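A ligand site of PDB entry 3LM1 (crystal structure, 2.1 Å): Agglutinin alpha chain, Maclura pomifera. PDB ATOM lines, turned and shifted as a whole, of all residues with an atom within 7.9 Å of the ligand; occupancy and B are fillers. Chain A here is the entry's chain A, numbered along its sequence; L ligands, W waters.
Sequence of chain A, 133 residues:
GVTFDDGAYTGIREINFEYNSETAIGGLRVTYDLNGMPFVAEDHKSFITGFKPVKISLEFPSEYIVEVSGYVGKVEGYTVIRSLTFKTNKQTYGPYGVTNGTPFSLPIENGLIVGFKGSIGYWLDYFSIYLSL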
ATOM      1  N   GLY A   1      -4.617   9.748  -4.326  1.00  0.00           N
ATOM      2  CA  GLY A   1      -3.991   9.315  -5.607  1.00  0.00           C
ATOM      3  C   GLY A   1      -2.869   8.318  -5.380  1.00  0.00           C
ATOM      4  O   GLY A   1      -2.690   7.834  -4.275  1.00  0.00           O
ATOM      5  N   VAL A   2      -2.130   8.002  -6.434  1.00  0.00           N
ATOM      6  CA  VAL A   2      -1.024   7.067  -6.353  1.00  0.00           C
ATOM      7  C   VAL A   2       0.293   7.832  -6.238  1.00  0.00           C
ATOM      8  O   VAL A   2       0.613   8.680  -7.078  1.00  0.00           O
ATOM      9  CB  VAL A   2      -0.967   6.170  -7.611  1.00  0.00           C
ATOM     10  CG1 VAL A   2       0.282   5.282  -7.569  1.00  0.00           C
ATOM     11  CG2 VAL A   2      -2.219   5.316  -7.711  1.00  0.00           C
ATOM     12  N   ALA A  24      -7.224  21.014 -13.539  1.00  0.00           N
ATOM     13  CA  ALA A  24      -5.902  21.145 -12.934  1.00  0.00           C
ATOM     14  C   ALA A  24      -4.836  20.369 -13.678  1.00  0.00           C
ATOM     15  O   ALA A  24      -5.057  19.882 -14.799  1.00  0.00           O
ATOM     16  CB  ALA A  24      -5.966  20.656 -11.488  1.00  0.00           C
ATOM     17  N   ILE A  25      -3.654  20.272 -13.054  1.00  0.00           N
ATOM     18  CA  ILE A  25      -2.527  19.548 -13.626  1.00  0.00           C
ATOM     19  C   ILE A  25      -2.818  18.051 -13.605  1.00  0.00           C
ATOM     20  O   ILE A  25      -3.385  17.531 -12.626  1.00  0.00           O
ATOM     21  CB  ILE A  25      -1.219  19.797 -12.833  1.00  0.00           C
ATOM     22  CG1 ILE A  25      -0.871  21.294 -12.868  1.00  0.00           C
ATOM     23  CG2 ILE A  25      -0.072  18.965 -13.413  1.00  0.00           C
ATOM     24  CD1 ILE A  25      -0.811  21.901 -14.279  1.00  0.00           C
ATOM     25  N   SER A  46      -2.317  10.307 -14.984  1.00  0.00           N
ATOM     26  CA  SER A  46      -3.536  10.706 -14.329  1.00  0.00           C
ATOM     27  C   SER A  46      -4.486   9.523 -14.483  1.00  0.00           C
ATOM     28  O   SER A  46      -4.285   8.678 -15.365  1.00  0.00           O
ATOM     29  CB  SER A  46      -4.147  11.909 -15.033  1.00  0.00           C
ATOM     30  OG  SER A  46      -5.536  11.971 -14.800  1.00  0.00           O
ATOM     31  N   PHE A  47      -5.518   9.473 -13.647  1.00  0.00           N
ATOM     32  CA  PHE A  47      -6.508   8.406 -13.730  1.00  0.00           C
ATOM     33  C   PHE A  47      -7.432   8.628 -14.926  1.00  0.00           C
ATOM     34  O   PHE A  47      -8.096   7.690 -15.377  1.00  0.00           O
ATOM     35  CB  PHE A  47      -7.398   8.358 -12.475  1.00  0.00           C
ATOM     36  CG  PHE A  47      -6.697   7.895 -11.228  1.00  0.00           C
ATOM     37  CD1 PHE A  47      -7.394   7.836 -10.020  1.00  0.00           C
ATOM     38  CD2 PHE A  47      -5.356   7.534 -11.238  1.00  0.00           C
ATOM     39  CE1 PHE A  47      -6.769   7.433  -8.840  1.00  0.00           C
ATOM     40  CE2 PHE A  47      -4.710   7.121 -10.054  1.00  0.00           C
ATOM     41  CZ  PHE A  47      -5.420   7.077  -8.852  1.00  0.00           C
ATOM     42  N   ILE A  48      -7.498   9.864 -15.407  1.00  0.00           N
ATOM     43  CA  ILE A  48      -8.379  10.191 -16.530  1.00  0.00           C
ATOM     44  C   ILE A  48      -7.622  10.812 -17.706  1.00  0.00           C
ATOM     45  O   ILE A  48      -6.410  10.991 -17.655  1.00  0.00           O
ATOM     46  CB  ILE A  48      -9.485  11.188 -16.091  1.00  0.00           C
ATOM     47  CG1 ILE A  48      -8.845  12.460 -15.535  1.00  0.00           C
ATOM     48  CG2 ILE A  48     -10.401  10.541 -15.061  1.00  0.00           C
ATOM     49  CD1 ILE A  48      -9.833  13.563 -15.236  1.00  0.00           C
ATOM     50  N   VAL A  75     -10.794  21.028  -6.769  1.00  0.00           N
ATOM     51  CA  VAL A  75     -11.472  20.582  -7.974  1.00  0.00           C
ATOM     52  C   VAL A  75     -12.248  19.341  -7.552  1.00  0.00           C
ATOM     53  O   VAL A  75     -11.649  18.367  -7.092  1.00  0.00           O
ATOM     54  CB  VAL A  75     -10.474  20.218  -9.095  1.00  0.00           C
ATOM     55  CG1 VAL A  75     -11.221  19.683 -10.313  1.00  0.00           C
ATOM     56  CG2 VAL A  75      -9.649  21.453  -9.495  1.00  0.00           C
ATOM     57  N   GLU A  76     -13.569  19.386  -7.665  1.00  0.00           N
ATOM     58  CA  GLU A  76     -14.405  18.265  -7.260  1.00  0.00           C
ATOM     59  C   GLU A  76     -14.144  17.956  -5.788  1.00  0.00           C
ATOM     60  O   GLU A  76     -14.186  16.792  -5.379  1.00  0.00           O
ATOM     61  CB  GLU A  76     -14.096  17.044  -8.123  1.00  0.00           C
ATOM     62  CG  GLU A  76     -14.278  17.306  -9.600  1.00  0.00           C
ATOM     63  CD  GLU A  76     -15.706  17.113 -10.052  1.00  0.00           C
ATOM     64  OE1 GLU A  76     -16.044  15.970 -10.427  1.00  0.00           O
ATOM     65  OE2 GLU A  76     -16.502  18.071 -10.025  1.00  0.00           O
ATOM     66  N   GLY A  77     -13.871  18.993  -5.012  1.00  0.00           N
ATOM     67  CA  GLY A  77     -13.629  18.839  -3.586  1.00  0.00           C
ATOM     68  C   GLY A  77     -12.209  18.487  -3.166  1.00  0.00           C
ATOM     69  O   GLY A  77     -11.868  18.582  -1.986  1.00  0.00           O
ATOM     70  N   TYR A  78     -11.377  18.088  -4.110  1.00  0.00           N
ATOM     71  CA  TYR A  78     -10.002  17.706  -3.806  1.00  0.00           C
ATOM     72  C   TYR A  78      -9.015  18.859  -4.002  1.00  0.00           C
ATOM     73  O   TYR A  78      -9.095  19.596  -4.983  1.00  0.00           O
ATOM     74  CB  TYR A  78      -9.550  16.527  -4.683  1.00  0.00           C
ATOM     75  CG  TYR A  78     -10.381  15.262  -4.543  1.00  0.00           C
ATOM     76  CD1 TYR A  78     -11.518  15.059  -5.332  1.00  0.00           C
ATOM     77  CD2 TYR A  78     -10.030  14.273  -3.627  1.00  0.00           C
ATOM     78  CE1 TYR A  78     -12.277  13.896  -5.219  1.00  0.00           C
ATOM     79  CE2 TYR A  78     -10.782  13.107  -3.501  1.00  0.00           C
ATOM     80  CZ  TYR A  78     -11.900  12.927  -4.302  1.00  0.00           C
ATOM     81  OH  TYR A  78     -12.630  11.769  -4.203  1.00  0.00           O
ATOM     82  N   THR A  79      -8.086  18.983  -3.059  1.00  0.00           N
ATOM     83  CA  THR A  79      -7.055  20.013  -3.114  1.00  0.00           C
ATOM     84  C   THR A  79      -5.938  19.469  -3.985  1.00  0.00           C
ATOM     85  O   THR A  79      -5.290  18.475  -3.639  1.00  0.00           O
ATOM     86  CB  THR A  79      -6.514  20.333  -1.714  1.00  0.00           C
ATOM     87  OG1 THR A  79      -7.583  20.802  -0.888  1.00  0.00           O
ATOM     88  CG2 THR A  79      -5.432  21.412  -1.783  1.00  0.00           C
ATOM     89  N   VAL A  80      -5.730  20.099  -5.140  1.00  0.00           N
ATOM     90  CA  VAL A  80      -4.726  19.651  -6.082  1.00  0.00           C
ATOM     91  C   VAL A  80      -3.949  20.825  -6.704  1.00  0.00           C
ATOM     92  O   VAL A  80      -4.324  21.992  -6.537  1.00  0.00           O
ATOM     93  CB  VAL A  80      -5.389  18.876  -7.229  1.00  0.00           C
ATOM     94  CG1 VAL A  80      -6.137  17.647  -6.704  1.00  0.00           C
ATOM     95  CG2 VAL A  80      -6.377  19.796  -7.944  1.00  0.00           C
ATOM     96  N   ILE A  81      -2.860  20.498  -7.418  1.00  0.00           N
ATOM     97  CA  ILE A  81      -2.075  21.520  -8.094  1.00  0.00           C
ATOM     98  C   ILE A  81      -2.838  21.854  -9.369  1.00  0.00           C
ATOM     99  O   ILE A  81      -3.009  21.004 -10.254  1.00  0.00           O
ATOM    100  CB  ILE A  81      -0.646  21.032  -8.424  1.00  0.00           C
ATOM    101  CG1 ILE A  81       0.199  20.925  -7.155  1.00  0.00           C
ATOM    102  CG2 ILE A  81       0.062  22.038  -9.353  1.00  0.00           C
ATOM    103  CD1 ILE A  81      -0.297  19.920  -6.150  1.00  0.00           C
ATOM    104  N   SER A 119       2.193  12.722  -5.737  1.00  0.00           N
ATOM    105  CA  SER A 119       1.037  11.841  -5.830  1.00  0.00           C
ATOM    106  C   SER A 119       0.116  12.331  -6.937  1.00  0.00           C
ATOM    107  O   SER A 119      -0.071  13.523  -7.086  1.00  0.00           O
ATOM    108  CB  SER A 119       0.267  11.839  -4.502  1.00  0.00           C
ATOM    109  OG  SER A 119      -0.984  11.181  -4.656  1.00  0.00           O
ATOM    110  N   ILE A 120      -0.449  11.404  -7.693  1.00  0.00           N
ATOM    111  CA  ILE A 120      -1.366  11.778  -8.759  1.00  0.00           C
ATOM    112  C   ILE A 120      -2.592  10.870  -8.815  1.00  0.00           C
ATOM    113  O   ILE A 120      -2.478   9.640  -8.844  1.00  0.00           O
ATOM    114  CB  ILE A 120      -0.673  11.740 -10.132  1.00  0.00           C
ATOM    115  CG1 ILE A 120       0.562  12.658 -10.103  1.00  0.00           C
ATOM    116  CG2 ILE A 120      -1.633  12.211 -11.207  1.00  0.00           C
ATOM    117  CD1 ILE A 120       1.327  12.725 -11.427  1.00  0.00           C
ATOM    118  N   GLY A 121      -3.767  11.487  -8.806  1.00  0.00           N
ATOM    119  CA  GLY A 121      -5.009  10.751  -8.904  1.00  0.00           C
ATOM    120  C   GLY A 121      -5.565  11.216 -10.236  1.00  0.00           C
ATOM    121  O   GLY A 121      -4.944  10.972 -11.273  1.00  0.00           O
ATOM    122  N   TYR A 122      -6.703  11.896 -10.213  1.00  0.00           N
ATOM    123  CA  TYR A 122      -7.264  12.437 -11.446  1.00  0.00           C
ATOM    124  C   TYR A 122      -6.299  13.556 -11.812  1.00  0.00           C
ATOM    125  O   TYR A 122      -6.001  13.779 -12.987  1.00  0.00           O
ATOM    126  CB  TYR A 122      -8.660  13.039 -11.201  1.00  0.00           C
ATOM    127  CG  TYR A 122      -9.823  12.098 -11.431  1.00  0.00           C
ATOM    128  CD1 TYR A 122      -9.808  10.800 -10.932  1.00  0.00           C
ATOM    129  CD2 TYR A 122     -10.974  12.543 -12.091  1.00  0.00           C
ATOM    130  CE1 TYR A 122     -10.922   9.964 -11.068  1.00  0.00           C
ATOM    131  CE2 TYR A 122     -12.086  11.715 -12.242  1.00  0.00           C
ATOM    132  CZ  TYR A 122     -12.048  10.429 -11.728  1.00  0.00           C
ATOM    133  OH  TYR A 122     -13.144   9.620 -11.866  1.00  0.00           O
ATOM    134  N   TRP A 123      -5.791  14.236 -10.790  1.00  0.00           N
ATOM    135  CA  TRP A 123      -4.861  15.339 -10.961  1.00  0.00           C
ATOM    136  C   TRP A 123      -3.677  15.254 -10.013  1.00  0.00           C
ATOM    137  O   TRP A 123      -3.646  14.420  -9.107  1.00  0.00           O
ATOM    138  CB  TRP A 123      -5.623  16.659 -10.746  1.00  0.00           C
ATOM    139  CG  TRP A 123      -6.859  16.747 -11.583  1.00  0.00           C
ATOM    140  CD1 TRP A 123      -6.905  16.880 -12.954  1.00  0.00           C
ATOM    141  CD2 TRP A 123      -8.212  16.593 -11.158  1.00  0.00           C
ATOM    142  NE1 TRP A 123      -8.222  16.814 -13.380  1.00  0.00           N
ATOM    143  CE2 TRP A 123      -9.028  16.629 -12.297  1.00  0.00           C
ATOM    144  CE3 TRP A 123      -8.807  16.412  -9.889  1.00  0.00           C
ATOM    145  CZ2 TRP A 123     -10.428  16.494 -12.229  1.00  0.00           C
ATOM    146  CZ3 TRP A 123     -10.185  16.280  -9.823  1.00  0.00           C
ATOM    147  CH2 TRP A 123     -10.986  16.318 -10.986  1.00  0.00           C
ATOM    148  N   LEU A 124      -2.690  16.110 -10.241  1.00  0.00           N
ATOM    149  CA  LEU A 124      -1.507  16.150  -9.381  1.00  0.00           C
ATOM    150  C   LEU A 124      -1.977  16.596  -7.981  1.00  0.00           C
ATOM    151  O   LEU A 124      -2.384  17.742  -7.804  1.00  0.00           O
ATOM    152  CB  LEU A 124      -0.484  17.157  -9.941  1.00  0.00           C
ATOM    153  CG  LEU A 124       0.825  17.315  -9.173  1.00  0.00           C
ATOM    154  CD1 LEU A 124       1.549  15.973  -9.102  1.00  0.00           C
ATOM    155  CD2 LEU A 124       1.673  18.376  -9.847  1.00  0.00           C
ATOM    156  N   ASP A 125      -1.906  15.701  -7.006  1.00  0.00           N
ATOM    157  CA  ASP A 125      -2.357  16.023  -5.650  1.00  0.00           C
ATOM    158  C   ASP A 125      -1.368  16.915  -4.930  1.00  0.00           C
ATOM    159  O   ASP A 125      -1.748  17.876  -4.267  1.00  0.00           O
ATOM    160  CB  ASP A 125      -2.560  14.746  -4.833  1.00  0.00           C
ATOM    161  CG  ASP A 125      -3.435  13.751  -5.534  1.00  0.00           C
ATOM    162  OD1 ASP A 125      -4.598  14.116  -5.873  1.00  0.00           O
ATOM    163  OD2 ASP A 125      -2.992  12.603  -5.756  1.00  0.00           O
ATOM    164  N   TYR A 126      -0.093  16.578  -5.047  1.00  0.00           N
ATOM    165  CA  TYR A 126       0.972  17.347  -4.418  1.00  0.00           C
ATOM    166  C   TYR A 126       2.296  16.846  -4.967  1.00  0.00           C
ATOM    167  O   TYR A 126       2.338  15.818  -5.652  1.00  0.00           O
ATOM    168  CB  TYR A 126       0.944  17.163  -2.890  1.00  0.00           C
ATOM    169  CG  TYR A 126       1.018  15.735  -2.401  1.00  0.00           C
ATOM    170  CD1 TYR A 126      -0.141  15.049  -2.010  1.00  0.00           C
ATOM    171  CD2 TYR A 126       2.240  15.065  -2.301  1.00  0.00           C
ATOM    172  CE1 TYR A 126      -0.080  13.726  -1.535  1.00  0.00           C
ATOM    173  CE2 TYR A 126       2.310  13.748  -1.828  1.00  0.00           C
ATOM    174  CZ  TYR A 126       1.155  13.087  -1.450  1.00  0.00           C
ATOM    175  OH  TYR A 126       1.227  11.787  -1.007  1.00  0.00           O
HETATM  176  C1  LIG L   1      -9.028   6.535  -4.593  1.00  0.00           C
HETATM  177  C2  LIG L   1      -8.248   7.741  -5.109  1.00  0.00           C
HETATM  178  O1  LIG L   1      -7.023   7.636  -5.283  1.00  0.00           O
HETATM  179  N1  LIG L   1      -8.905   8.885  -5.369  1.00  0.00           N
HETATM  180  C3  LIG L   1      -8.212  10.085  -5.857  1.00  0.00           C
HETATM  181  C4  LIG L   1      -8.076  11.158  -4.752  1.00  0.00           C
HETATM  182  O2  LIG L   1      -7.355  10.622  -3.626  1.00  0.00           O
HETATM  183  C5  LIG L   1      -7.348  12.394  -5.323  1.00  0.00           C
HETATM  184  O3  LIG L   1      -6.043  11.975  -5.732  1.00  0.00           O
HETATM  185  C6  LIG L   1      -8.151  12.948  -6.540  1.00  0.00           C
HETATM  186  C7  LIG L   1      -7.470  14.194  -7.157  1.00  0.00           C
HETATM  187  O4  LIG L   1      -6.379  13.823  -7.984  1.00  0.00           O
HETATM  188  O5  LIG L   1      -8.306  11.895  -7.555  1.00  0.00           O
HETATM  189  C8  LIG L   1      -8.975  10.666  -7.055  1.00  0.00           C
HETATM  190  O6  LIG L   1     -10.315  10.985  -6.687  1.00  0.00           O
HETATM  191  C9  LIG L   1     -11.419  11.394  -7.498  1.00  0.00           C
HETATM  192  C10 LIG L   1     -12.582  10.566  -7.581  1.00  0.00           C
HETATM  193  C11 LIG L   1     -13.671  10.977  -8.382  1.00  0.00           C
HETATM  194  C12 LIG L   1     -13.625  12.220  -9.101  1.00  0.00           C
HETATM  195  N2  LIG L   1     -14.702  12.616  -9.896  1.00  0.00           N
HETATM  196  O7  LIG L   1     -14.665  13.708 -10.536  1.00  0.00           O
HETATM  197  O8  LIG L   1     -15.720  11.900  -9.992  1.00  0.00           O
HETATM  198  C13 LIG L   1     -12.464  13.036  -9.012  1.00  0.00           C
HETATM  199  C14 LIG L   1     -11.366  12.630  -8.213  1.00  0.00           C
HETATM  200  O   HOH W   1      -9.661   9.443  -2.362  1.00  0.00           O
HETATM  201  O   HOH W   2      -6.698  13.481  -1.925  1.00  0.00           O
HETATM  202  O   HOH W   3      -5.313   5.589  -5.360  1.00  0.00           O
HETATM  203  O   HOH W   4     -15.289  13.360 -13.398  1.00  0.00           O
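OD2 of Asp 125 sits at hydrogen-bond distance from N of Ile 120 (3.4 Å).
The backbone NH (N) of Gly 121 is in hydrogen-bond range of the side-chain carboxylate (OD2) of Asp 125.
The backbone NH (N) of Phe 47 is in hydrogen-bond range of the backbone carbonyl oxygen (O) of Gly 121.
OG of Ser 46 lies within hydrogen-bond range of O of Tyr 122, 2.6 Å away.
The side-chain hydroxyl of Ser 119 is in hydrogen-bond range of the side-chain carboxylate of Asp 125, 2.7 Å away.
The backbone carbonyl oxygen of Trp 123 is in hydrogen-bond range of an oxygen (O4) of the ligand (3.0 Å).
An oxygen (O7) of the ligand lies close to the side-chain carboxylate (OE1) of Glu 76 (2.7 Å).
N of Tyr 122 is in hydrogen-bond range of O4 of the ligand (3.0 Å).
O4 of the ligand lies within hydrogen-bond range of N of Trp 123.
An oxygen (O3) of the ligand lies within hydrogen-bond range of the side-chain carboxylate of Asp 125 (2.6 Å).
The backbone NH (N) of Gly 1 is in hydrogen-bond range of an oxygen (O2) of the ligand (3.0 Å).
The side-chain hydroxyl (OH) of Tyr 78 sits close to an oxygen (O6) of the ligand, at 3.5 Å.
Merely in contact with the ligand: Phe 47 (3.6 Å), Val 80 (3.7 Å) and Gly 121 (3.5 Å).
Along chain A the residues within 4 Å of the ligand span positions 1 to 125.
The nearest printed residue that does not touch the ligand is Ile 120 (4.8 Å).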
